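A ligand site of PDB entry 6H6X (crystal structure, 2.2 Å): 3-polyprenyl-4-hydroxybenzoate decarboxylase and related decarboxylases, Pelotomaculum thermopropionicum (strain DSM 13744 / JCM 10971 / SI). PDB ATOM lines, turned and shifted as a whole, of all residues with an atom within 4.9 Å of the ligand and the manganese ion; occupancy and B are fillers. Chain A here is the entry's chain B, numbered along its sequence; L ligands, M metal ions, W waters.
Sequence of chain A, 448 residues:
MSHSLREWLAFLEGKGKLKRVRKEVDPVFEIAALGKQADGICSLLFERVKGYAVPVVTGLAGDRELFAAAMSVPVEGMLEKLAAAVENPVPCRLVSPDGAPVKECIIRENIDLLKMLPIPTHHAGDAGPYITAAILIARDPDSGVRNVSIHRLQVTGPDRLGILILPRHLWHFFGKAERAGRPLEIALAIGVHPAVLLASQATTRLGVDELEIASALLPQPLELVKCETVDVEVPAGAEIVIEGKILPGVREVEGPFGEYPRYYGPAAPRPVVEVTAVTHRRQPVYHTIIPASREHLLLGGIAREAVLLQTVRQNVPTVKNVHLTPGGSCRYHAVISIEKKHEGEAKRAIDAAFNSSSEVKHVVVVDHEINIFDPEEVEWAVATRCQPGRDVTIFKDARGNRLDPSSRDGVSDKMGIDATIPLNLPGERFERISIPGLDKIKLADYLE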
ATOM      1  N   THR A 132      24.149  -3.177  12.580  1.00  0.00           N
ATOM      2  CA  THR A 132      23.618  -3.520  13.889  1.00  0.00           C
ATOM      3  C   THR A 132      22.261  -4.165  13.884  1.00  0.00           C
ATOM      4  O   THR A 132      21.806  -4.596  14.945  1.00  0.00           O
ATOM      5  CB  THR A 132      23.505  -2.272  14.767  1.00  0.00           C
ATOM      6  OG1 THR A 132      22.722  -1.283  14.079  1.00  0.00           O
ATOM      7  CG2 THR A 132      24.881  -1.704  15.070  1.00  0.00           C
ATOM      8  N   ASN A 147      20.060 -21.848  12.817  1.00  0.00           N
ATOM      9  CA  ASN A 147      20.014 -20.849  13.910  1.00  0.00           C
ATOM     10  C   ASN A 147      19.977 -19.434  13.337  1.00  0.00           C
ATOM     11  O   ASN A 147      20.507 -19.165  12.253  1.00  0.00           O
ATOM     12  CB  ASN A 147      21.263 -21.017  14.746  1.00  0.00           C
ATOM     13  CG  ASN A 147      21.138 -20.408  16.095  1.00  0.00           C
ATOM     14  OD1 ASN A 147      20.495 -21.009  16.980  1.00  0.00           O
ATOM     15  ND2 ASN A 147      21.783 -19.202  16.304  1.00  0.00           N
ATOM     16  N   VAL A 148      19.371 -18.537  14.091  1.00  0.00           N
ATOM     17  CA  VAL A 148      19.351 -17.120  13.803  1.00  0.00           C
ATOM     18  C   VAL A 148      19.807 -16.380  15.072  1.00  0.00           C
ATOM     19  O   VAL A 148      19.361 -16.692  16.153  1.00  0.00           O
ATOM     20  CB  VAL A 148      17.947 -16.659  13.438  1.00  0.00           C
ATOM     21  CG1 VAL A 148      17.944 -15.230  12.937  1.00  0.00           C
ATOM     22  CG2 VAL A 148      17.379 -17.577  12.355  1.00  0.00           C
ATOM     23  N   SER A 149      20.651 -15.367  14.911  1.00  0.00           N
ATOM     24  CA  SER A 149      21.095 -14.458  15.966  1.00  0.00           C
ATOM     25  C   SER A 149      21.517 -13.117  15.355  1.00  0.00           C
ATOM     26  O   SER A 149      21.686 -12.989  14.135  1.00  0.00           O
ATOM     27  CB  SER A 149      22.276 -15.081  16.745  1.00  0.00           C
ATOM     28  OG  SER A 149      23.208 -15.722  15.873  1.00  0.00           O
ATOM     29  N   ILE A 150      21.683 -12.105  16.188  1.00  0.00           N
ATOM     30  CA  ILE A 150      22.104 -10.786  15.728  1.00  0.00           C
ATOM     31  C   ILE A 150      23.493 -10.523  16.312  1.00  0.00           C
ATOM     32  O   ILE A 150      23.688 -10.615  17.541  1.00  0.00           O
ATOM     33  CB  ILE A 150      21.122  -9.682  16.173  1.00  0.00           C
ATOM     34  CG1 ILE A 150      19.785  -9.887  15.461  1.00  0.00           C
ATOM     35  CG2 ILE A 150      21.686  -8.301  15.858  1.00  0.00           C
ATOM     36  CD1 ILE A 150      18.732  -8.822  15.787  1.00  0.00           C
ATOM     37  N   HIS A 151      24.413 -10.160  15.428  1.00  0.00           N
ATOM     38  CA  HIS A 151      25.821  -9.848  15.788  1.00  0.00           C
ATOM     39  C   HIS A 151      26.208  -8.515  15.177  1.00  0.00           C
ATOM     40  O   HIS A 151      25.792  -8.189  14.059  1.00  0.00           O
ATOM     41  CB  HIS A 151      26.763 -10.944  15.244  1.00  0.00           C
ATOM     42  CG  HIS A 151      26.399 -12.301  15.735  1.00  0.00           C
ATOM     43  ND1 HIS A 151      26.946 -12.856  16.877  1.00  0.00           N
ATOM     44  CD2 HIS A 151      25.407 -13.158  15.339  1.00  0.00           C
ATOM     45  CE1 HIS A 151      26.337 -14.008  17.131  1.00  0.00           C
ATOM     46  NE2 HIS A 151      25.413 -14.212  16.203  1.00  0.00           N
ATOM     47  N   ARG A 152      26.941  -7.707  15.938  1.00  0.00           N
ATOM     48  CA  ARG A 152      27.499  -6.487  15.355  1.00  0.00           C
ATOM     49  C   ARG A 152      28.549  -6.844  14.316  1.00  0.00           C
ATOM     50  O   ARG A 152      29.292  -7.800  14.485  1.00  0.00           O
ATOM     51  CB  ARG A 152      28.040  -5.558  16.448  1.00  0.00           C
ATOM     52  CG  ARG A 152      29.339  -6.019  17.045  1.00  0.00           C
ATOM     53  CD  ARG A 152      29.764  -5.159  18.212  1.00  0.00           C
ATOM     54  NE  ARG A 152      31.141  -5.459  18.615  1.00  0.00           N
ATOM     55  CZ  ARG A 152      31.639  -5.441  19.860  1.00  0.00           C
ATOM     56  NH1 ARG A 152      30.915  -5.165  20.922  1.00  0.00           N
ATOM     57  NH2 ARG A 152      32.909  -5.751  20.022  1.00  0.00           N
ATOM     58  N   LEU A 164      31.668  -9.930  16.182  1.00  0.00           N
ATOM     59  CA  LEU A 164      31.706 -10.378  17.540  1.00  0.00           C
ATOM     60  C   LEU A 164      30.773 -11.571  17.662  1.00  0.00           C
ATOM     61  O   LEU A 164      29.567 -11.428  17.432  1.00  0.00           O
ATOM     62  CB  LEU A 164      31.246  -9.254  18.484  1.00  0.00           C
ATOM     63  CG  LEU A 164      30.976  -9.762  19.941  1.00  0.00           C
ATOM     64  CD1 LEU A 164      32.273 -10.287  20.565  1.00  0.00           C
ATOM     65  CD2 LEU A 164      30.351  -8.668  20.775  1.00  0.00           C
ATOM     66  N   ILE A 165      31.311 -12.747  17.990  1.00  0.00           N
ATOM     67  CA  ILE A 165      30.509 -13.918  18.285  1.00  0.00           C
ATOM     68  C   ILE A 165      30.714 -14.336  19.771  1.00  0.00           C
ATOM     69  O   ILE A 165      31.736 -14.873  20.151  1.00  0.00           O
ATOM     70  CB  ILE A 165      30.854 -15.096  17.351  1.00  0.00           C
ATOM     71  CG1 ILE A 165      30.942 -14.638  15.880  1.00  0.00           C
ATOM     72  CG2 ILE A 165      29.820 -16.200  17.433  1.00  0.00           C
ATOM     73  CD1 ILE A 165      31.304 -15.782  14.944  1.00  0.00           C
ATOM     74  N   LEU A 166      29.704 -14.120  20.594  1.00  0.00           N
ATOM     75  CA  LEU A 166      29.683 -14.630  21.960  1.00  0.00           C
ATOM     76  C   LEU A 166      29.524 -16.151  21.986  1.00  0.00           C
ATOM     77  O   LEU A 166      29.071 -16.737  21.008  1.00  0.00           O
ATOM     78  CB  LEU A 166      28.607 -13.901  22.764  1.00  0.00           C
ATOM     79  CG  LEU A 166      28.906 -12.382  22.909  1.00  0.00           C
ATOM     80  CD1 LEU A 166      27.776 -11.601  23.588  1.00  0.00           C
ATOM     81  CD2 LEU A 166      30.232 -12.147  23.676  1.00  0.00           C
ATOM     82  N   ARG A 168      27.769 -18.919  22.223  1.00  0.00           N
ATOM     83  CA  ARG A 168      26.364 -19.355  22.180  1.00  0.00           C
ATOM     84  C   ARG A 168      26.217 -20.222  20.905  1.00  0.00           C
ATOM     85  O   ARG A 168      27.182 -20.901  20.541  1.00  0.00           O
ATOM     86  CB  ARG A 168      25.418 -18.132  22.185  1.00  0.00           C
ATOM     87  CG  ARG A 168      25.351 -17.266  23.458  1.00  0.00           C
ATOM     88  CD  ARG A 168      24.453 -17.886  24.552  1.00  0.00           C
ATOM     89  NE  ARG A 168      23.141 -18.369  24.060  1.00  0.00           N
ATOM     90  CZ  ARG A 168      22.521 -19.505  24.387  1.00  0.00           C
ATOM     91  NH1 ARG A 168      23.041 -20.361  25.260  1.00  0.00           N
ATOM     92  NH2 ARG A 168      21.349 -19.802  23.833  1.00  0.00           N
ATOM     93  N   HIS A 169      25.082 -20.209  20.175  1.00  0.00           N
ATOM     94  CA  HIS A 169      24.930 -21.170  19.085  1.00  0.00           C
ATOM     95  C   HIS A 169      25.814 -20.976  17.856  1.00  0.00           C
ATOM     96  O   HIS A 169      26.380 -21.920  17.346  1.00  0.00           O
ATOM     97  CB  HIS A 169      23.461 -21.335  18.692  1.00  0.00           C
ATOM     98  CG  HIS A 169      22.623 -21.843  19.816  1.00  0.00           C
ATOM     99  ND1 HIS A 169      21.257 -21.656  19.875  1.00  0.00           N
ATOM    100  CD2 HIS A 169      22.961 -22.486  20.964  1.00  0.00           C
ATOM    101  CE1 HIS A 169      20.790 -22.194  20.993  1.00  0.00           C
ATOM    102  NE2 HIS A 169      21.803 -22.696  21.673  1.00  0.00           N
ATOM    103  N   LEU A 170      25.936 -19.745  17.358  1.00  0.00           N
ATOM    104  CA  LEU A 170      26.756 -19.543  16.192  1.00  0.00           C
ATOM    105  C   LEU A 170      28.232 -19.950  16.454  1.00  0.00           C
ATOM    106  O   LEU A 170      28.885 -20.496  15.605  1.00  0.00           O
ATOM    107  CB  LEU A 170      26.695 -18.083  15.795  1.00  0.00           C
ATOM    108  CG  LEU A 170      27.479 -17.759  14.539  1.00  0.00           C
ATOM    109  CD1 LEU A 170      26.962 -18.541  13.377  1.00  0.00           C
ATOM    110  CD2 LEU A 170      27.378 -16.281  14.294  1.00  0.00           C
ATOM    111  N   SER A 200      14.668 -13.715  16.672  1.00  0.00           N
ATOM    112  CA  SER A 200      16.123 -13.959  16.644  1.00  0.00           C
ATOM    113  C   SER A 200      16.795 -13.891  18.010  1.00  0.00           C
ATOM    114  O   SER A 200      17.951 -14.325  18.156  1.00  0.00           O
ATOM    115  CB  SER A 200      16.810 -12.971  15.729  1.00  0.00           C
ATOM    116  OG  SER A 200      16.859 -11.681  16.343  1.00  0.00           O
ATOM    117  N   GLN A 201      16.106 -13.304  18.989  1.00  0.00           N
ATOM    118  CA  GLN A 201      16.594 -13.178  20.356  1.00  0.00           C
ATOM    119  C   GLN A 201      16.133 -14.302  21.295  1.00  0.00           C
ATOM    120  O   GLN A 201      16.556 -14.308  22.434  1.00  0.00           O
ATOM    121  CB  GLN A 201      16.183 -11.794  20.903  1.00  0.00           C
ATOM    122  CG  GLN A 201      16.743 -10.672  20.059  1.00  0.00           C
ATOM    123  CD  GLN A 201      18.266 -10.783  19.961  1.00  0.00           C
ATOM    124  OE1 GLN A 201      18.834 -11.142  18.915  1.00  0.00           O
ATOM    125  NE2 GLN A 201      18.931 -10.554  21.076  1.00  0.00           N
ATOM    126  N   ALA A 202      15.332 -15.238  20.832  1.00  0.00           N
ATOM    127  CA  ALA A 202      15.039 -16.431  21.639  1.00  0.00           C
ATOM    128  C   ALA A 202      16.305 -17.221  22.013  1.00  0.00           C
ATOM    129  O   ALA A 202      17.193 -17.518  21.183  1.00  0.00           O
ATOM    130  CB  ALA A 202      14.054 -17.357  20.935  1.00  0.00           C
ATOM    131  N   THR A 203      16.357 -17.534  23.298  1.00  0.00           N
ATOM    132  CA  THR A 203      17.352 -18.370  23.906  1.00  0.00           C
ATOM    133  C   THR A 203      16.647 -19.699  24.070  1.00  0.00           C
ATOM    134  O   THR A 203      15.644 -19.833  24.787  1.00  0.00           O
ATOM    135  CB  THR A 203      17.791 -17.785  25.272  1.00  0.00           C
ATOM    136  OG1 THR A 203      18.243 -16.437  25.055  1.00  0.00           O
ATOM    137  CG2 THR A 203      18.933 -18.609  25.928  1.00  0.00           C
ATOM    138  N   THR A 204      17.162 -20.683  23.356  1.00  0.00           N
ATOM    139  CA  THR A 204      16.592 -22.010  23.341  1.00  0.00           C
ATOM    140  C   THR A 204      17.698 -23.046  23.528  1.00  0.00           C
ATOM    141  O   THR A 204      18.901 -22.698  23.518  1.00  0.00           O
ATOM    142  CB  THR A 204      15.881 -22.301  22.003  1.00  0.00           C
ATOM    143  OG1 THR A 204      16.837 -22.672  21.014  1.00  0.00           O
ATOM    144  CG2 THR A 204      15.092 -21.062  21.476  1.00  0.00           C
ATOM    145  N   VAL A 208      16.666 -25.532  17.946  1.00  0.00           N
ATOM    146  CA  VAL A 208      15.371 -24.994  17.480  1.00  0.00           C
ATOM    147  C   VAL A 208      15.604 -23.735  16.656  1.00  0.00           C
ATOM    148  O   VAL A 208      16.335 -22.808  17.030  1.00  0.00           O
ATOM    149  CB  VAL A 208      14.282 -24.832  18.577  1.00  0.00           C
ATOM    150  CG1 VAL A 208      14.781 -24.047  19.730  1.00  0.00           C
ATOM    151  CG2 VAL A 208      13.051 -24.146  18.053  1.00  0.00           C
ATOM    152  N   GLU A 210      15.132 -20.467  15.002  1.00  0.00           N
ATOM    153  CA  GLU A 210      14.421 -19.233  15.287  1.00  0.00           C
ATOM    154  C   GLU A 210      13.578 -18.717  14.113  1.00  0.00           C
ATOM    155  O   GLU A 210      12.625 -17.960  14.344  1.00  0.00           O
ATOM    156  CB  GLU A 210      15.335 -18.158  15.796  1.00  0.00           C
ATOM    157  CG  GLU A 210      15.871 -18.505  17.163  1.00  0.00           C
ATOM    158  CD  GLU A 210      17.251 -19.209  17.114  1.00  0.00           C
ATOM    159  OE1 GLU A 210      17.627 -19.790  16.107  1.00  0.00           O
ATOM    160  OE2 GLU A 210      17.960 -19.123  18.094  1.00  0.00           O
ATOM    161  N   PHE A 257      33.519  -0.810  20.361  1.00  0.00           N
ATOM    162  CA  PHE A 257      32.132  -0.459  19.973  1.00  0.00           C
ATOM    163  C   PHE A 257      31.313  -0.061  21.194  1.00  0.00           C
ATOM    164  O   PHE A 257      31.346  -0.755  22.212  1.00  0.00           O
ATOM    165  CB  PHE A 257      31.559  -1.708  19.289  1.00  0.00           C
ATOM    166  CG  PHE A 257      30.145  -1.595  18.810  1.00  0.00           C
ATOM    167  CD1 PHE A 257      29.826  -0.933  17.677  1.00  0.00           C
ATOM    168  CD2 PHE A 257      29.124  -2.213  19.519  1.00  0.00           C
ATOM    169  CE1 PHE A 257      28.517  -0.866  17.220  1.00  0.00           C
ATOM    170  CE2 PHE A 257      27.800  -2.186  19.058  1.00  0.00           C
ATOM    171  CZ  PHE A 257      27.521  -1.545  17.883  1.00  0.00           C
ATOM    172  N   GLU A 259      28.214  -0.358  23.427  1.00  0.00           N
ATOM    173  CA  GLU A 259      27.324  -1.522  23.607  1.00  0.00           C
ATOM    174  C   GLU A 259      26.089  -1.249  24.514  1.00  0.00           C
ATOM    175  O   GLU A 259      25.954  -0.166  25.044  1.00  0.00           O
ATOM    176  CB  GLU A 259      28.162  -2.697  24.169  1.00  0.00           C
ATOM    177  CG  GLU A 259      28.610  -3.754  23.159  1.00  0.00           C
ATOM    178  CD  GLU A 259      27.472  -4.527  22.450  1.00  0.00           C
ATOM    179  OE1 GLU A 259      27.846  -5.475  21.712  1.00  0.00           O
ATOM    180  OE2 GLU A 259      26.219  -4.230  22.589  1.00  0.00           O
ATOM    181  N   ILE A 289      19.851  -0.287  14.245  1.00  0.00           N
ATOM    182  CA  ILE A 289      19.456  -0.244  15.634  1.00  0.00           C
ATOM    183  C   ILE A 289      20.528   0.525  16.359  1.00  0.00           C
ATOM    184  O   ILE A 289      21.702   0.191  16.255  1.00  0.00           O
ATOM    185  CB  ILE A 289      19.294  -1.662  16.196  1.00  0.00           C
ATOM    186  CG1 ILE A 289      18.011  -2.307  15.683  1.00  0.00           C
ATOM    187  CG2 ILE A 289      19.329  -1.682  17.745  1.00  0.00           C
ATOM    188  CD1 ILE A 289      18.042  -3.831  15.849  1.00  0.00           C
ATOM    189  N   PRO A 291      22.731   1.396  19.351  1.00  0.00           N
ATOM    190  CA  PRO A 291      22.967   0.582  20.556  1.00  0.00           C
ATOM    191  C   PRO A 291      22.572   1.271  21.838  1.00  0.00           C
ATOM    192  O   PRO A 291      22.694   2.482  21.941  1.00  0.00           O
ATOM    193  CB  PRO A 291      24.476   0.352  20.514  1.00  0.00           C
ATOM    194  CG  PRO A 291      24.757   0.277  19.095  1.00  0.00           C
ATOM    195  CD  PRO A 291      23.931   1.393  18.511  1.00  0.00           C
ATOM    196  N   HIS A 296      16.920  -1.510  21.073  1.00  0.00           N
ATOM    197  CA  HIS A 296      17.937  -2.496  21.363  1.00  0.00           C
ATOM    198  C   HIS A 296      17.606  -3.243  22.640  1.00  0.00           C
ATOM    199  O   HIS A 296      17.572  -4.462  22.652  1.00  0.00           O
ATOM    200  CB  HIS A 296      19.298  -1.838  21.432  1.00  0.00           C
ATOM    201  CG  HIS A 296      20.412  -2.790  21.696  1.00  0.00           C
ATOM    202  ND1 HIS A 296      21.643  -2.366  22.152  1.00  0.00           N
ATOM    203  CD2 HIS A 296      20.499  -4.148  21.579  1.00  0.00           C
ATOM    204  CE1 HIS A 296      22.438  -3.402  22.305  1.00  0.00           C
ATOM    205  NE2 HIS A 296      21.767  -4.503  21.980  1.00  0.00           N
ATOM    206  N   LEU A 299      14.273  -5.500  22.448  1.00  0.00           N
ATOM    207  CA  LEU A 299      14.342  -6.691  21.585  1.00  0.00           C
ATOM    208  C   LEU A 299      14.857  -7.854  22.390  1.00  0.00           C
ATOM    209  O   LEU A 299      14.206  -8.875  22.433  1.00  0.00           O
ATOM    210  CB  LEU A 299      15.264  -6.532  20.361  1.00  0.00           C
ATOM    211  CG  LEU A 299      14.653  -6.109  19.055  1.00  0.00           C
ATOM    212  CD1 LEU A 299      15.739  -5.892  18.018  1.00  0.00           C
ATOM    213  CD2 LEU A 299      13.687  -7.177  18.584  1.00  0.00           C
ATOM    214  N   GLY A 300      16.017  -7.706  22.988  1.00  0.00           N
ATOM    215  CA  GLY A 300      16.587  -8.713  23.849  1.00  0.00           C
ATOM    216  C   GLY A 300      15.822  -8.933  25.146  1.00  0.00           C
ATOM    217  O   GLY A 300      15.602 -10.083  25.550  1.00  0.00           O
HETATM  218  C1  LIG L   1      21.475  -8.706  20.027  1.00  0.00           C
HETATM  219  C2  LIG L   1      20.846  -7.535  19.520  1.00  0.00           C
HETATM  220  C3  LIG L   1      21.580  -6.451  18.992  1.00  0.00           C
HETATM  221  C4  LIG L   1      24.935 -10.121  20.264  1.00  0.00           C
HETATM  222  C5  LIG L   1      23.044  -6.412  19.218  1.00  0.00           C
HETATM  223  N1  LIG L   1      27.498 -10.696  19.295  1.00  0.00           N
HETATM  224  C6  LIG L   1      26.734 -11.668  19.871  1.00  0.00           C
HETATM  225  C7  LIG L   1      23.689  -3.822  18.386  1.00  0.00           C
HETATM  226  C8  LIG L   1      23.985  -5.268  18.749  1.00  0.00           C
HETATM  227  C9  LIG L   1      25.842  -6.559  19.857  1.00  0.00           C
HETATM  228  O1  LIG L   1      27.224 -12.828  19.962  1.00  0.00           O
HETATM  229  N2  LIG L   1      25.475 -11.373  20.338  1.00  0.00           N
HETATM  230  C10 LIG L   1      27.050  -9.428  19.155  1.00  0.00           C
HETATM  231  O2  LIG L   1      27.763  -8.605  18.564  1.00  0.00           O
HETATM  232  C11 LIG L   1      25.667  -9.100  19.654  1.00  0.00           C
HETATM  233  N3  LIG L   1      25.074  -7.809  19.519  1.00  0.00           N
HETATM  234  C12 LIG L   1      25.345  -5.416  19.346  1.00  0.00           C
HETATM  235  C13 LIG L   1      24.232  -5.680  17.241  1.00  0.00           C
HETATM  236  C14 LIG L   1      23.667  -7.681  19.571  1.00  0.00           C
HETATM  237  C15 LIG L   1      20.919  -5.225  18.475  1.00  0.00           C
HETATM  238  C16 LIG L   1      19.336  -7.590  19.470  1.00  0.00           C
HETATM  239  C17 LIG L   1      22.866  -8.804  20.107  1.00  0.00           C
HETATM  240  N4  LIG L   1      23.607  -9.851  20.724  1.00  0.00           N
HETATM  241  C18 LIG L   1      22.892 -10.960  21.364  1.00  0.00           C
HETATM  242  C19 LIG L   1      22.405 -12.121  20.448  1.00  0.00           C
HETATM  243  O3  LIG L   1      21.834 -11.740  19.140  1.00  0.00           O
HETATM  244  C20 LIG L   1      21.368 -12.903  21.295  1.00  0.00           C
HETATM  245  O4  LIG L   1      21.819 -13.286  22.615  1.00  0.00           O
HETATM  246  C21 LIG L   1      20.995 -14.176  20.544  1.00  0.00           C
HETATM  247  O5  LIG L   1      19.755 -14.672  21.075  1.00  0.00           O
HETATM  248  C22 LIG L   1      22.024 -15.320  20.645  1.00  0.00           C
HETATM  249  O6  LIG L   1      21.391 -16.366  19.878  1.00  0.00           O
HETATM  250  P1  LIG L   1      21.673 -17.937  20.069  1.00  0.00           P
HETATM  251  O7  LIG L   1      21.031 -18.548  18.873  1.00  0.00           O
HETATM  252  O8  LIG L   1      23.199 -18.135  20.073  1.00  0.00           O
HETATM  253  O9  LIG L   1      21.042 -18.329  21.404  1.00  0.00           O
HETATM  254 MN    MN M   1      19.751 -20.385  18.758  1.00  0.00          MN
HETATM  255  O   HOH W   1      18.895 -19.638  20.844  1.00  0.00           O
HETATM  256  O   HOH W   2      18.307 -22.237  18.422  1.00  0.00           O
HETATM  257  O   HOH W   3      22.327 -11.754  24.873  1.00  0.00           O
HETATM  258  O   HOH W   4      24.531 -17.241  18.266  1.00  0.00           O
HETATM  259  O   HOH W   5      20.200 -16.365  23.271  1.00  0.00           O
HETATM  260  O   HOH W   6      23.070  -7.326  23.269  1.00  0.00           O
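O of Thr 204 sits close to NE2 of His 169 (3.4 Å). OE1 of Glu 210 sits at hydrogen-bond distance from N of Val 148 (2.9 Å). ND1 of His 151 lies within hydrogen-bond range of O of Leu 164, 3.0 Å away. OE1 of Glu 259 lies within salt-bridge range of NH1 of Arg 152 (3.2 Å). The side-chain amide oxygen (OE1) of Gln 201 lies within hydrogen-bond range of the side-chain hydroxyl (OG) of Ser 200, at 3.3 Å. NE2 of His 151 is in hydrogen-bond range of OG of Ser 149 (2.7 Å). O of Ile 289 is in hydrogen-bond range of OG1 of Thr 132 (2.8 Å).
Water W1 lies within hydrogen-bond range of O9 of the ligand (2.6 Å), O of Ala 202 (2.7 Å) and N of Thr 204 (3.2 Å). Water W2 lies within hydrogen-bond range of O of Val 208 (2.5 Å), OG1 of Thr 204 (3.0 Å) and OE1 of Glu 210 (3.4 Å). Water W4 lies within hydrogen-bond range of O8 of the ligand (2.4 Å), N of Leu 170 (3.0 Å) and OG of Ser 149 (3.1 Å). Water W5 lies within hydrogen-bond range of the side-chain hydroxyl of Thr 203 and an oxygen (O5) of the ligand.
N of His 169 is in hydrogen-bond range of O8 of the ligand, 2.8 Å away. N of Ile 150 is in hydrogen-bond range of O3 of the ligand. An oxygen (O3) of the ligand lies within hydrogen-bond range of the backbone carbonyl oxygen (O) of Ile 150. The guanidinium group of Arg 168 lies within salt-bridge range of an oxygen (O9) of the ligand, 2.9 Å away. N of Leu 166 is in hydrogen-bond range of O1 of the ligand. O of Leu 164 is in hydrogen-bond range of N1 of the ligand (2.9 Å). N of Arg 152 is in hydrogen-bond range of O2 of the ligand (2.9 Å). The backbone carbonyl oxygen of Gln 201 lies within hydrogen-bond range of an oxygen (O5) of the ligand. The side-chain amide oxygen (OE1) of Gln 201 lies within hydrogen-bond range of an oxygen (O3) of the ligand. An oxygen (O1) of the ligand lies within hydrogen-bond range of a ring nitrogen (ND1) of His 151 (3.1 Å). O5 of the ligand lies within hydrogen-bond range of O of Ser 200, 3.4 Å away.
The manganese ion is bound by the side-chain amide oxygen of Asn 147 (2.0 Å), an oxygen (O7) of the ligand (2.2 Å), a ring nitrogen (ND1) of His 169 (2.3 Å), the side-chain carboxylate of Glu 210 (2.3 Å), water W2 (2.4 Å) and water W1 (2.4 Å). The manganese ion has six donor atoms within binding distance.
Residues that only touch the ligand: Thr 132 (3.5 Å), Val 148 (3.7 Å), Ser 149 (3.5 Å), Ile 165 (3.8 Å), Ala 202 (3.8 Å), Glu 259 (2.9 Å), Ile 289 (3.95 Å) and His 296 (3.3 Å). Hydrophobic or aromatic side chains within 4 Å of the ligand: Ile 150, His 151, Leu 164, Leu 166, His 169, Ile 289 and His 296. Within 4 Å of the ligand: Thr 132, Asn 147, Val 148, Ser 149, Ile 150, His 151, Arg 152, Leu 164, Ile 165, Leu 166, Arg 168, His 169, Ser 200, Gln 201, Ala 202, Glu 210, Glu 259, Ile 289 and His 296.
Along chain A the residues within 4 Å of the manganese ion span positions 147 to 210. The nearest printed residue that does not touch the manganese ion is Thr 204 (4.3 Å).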
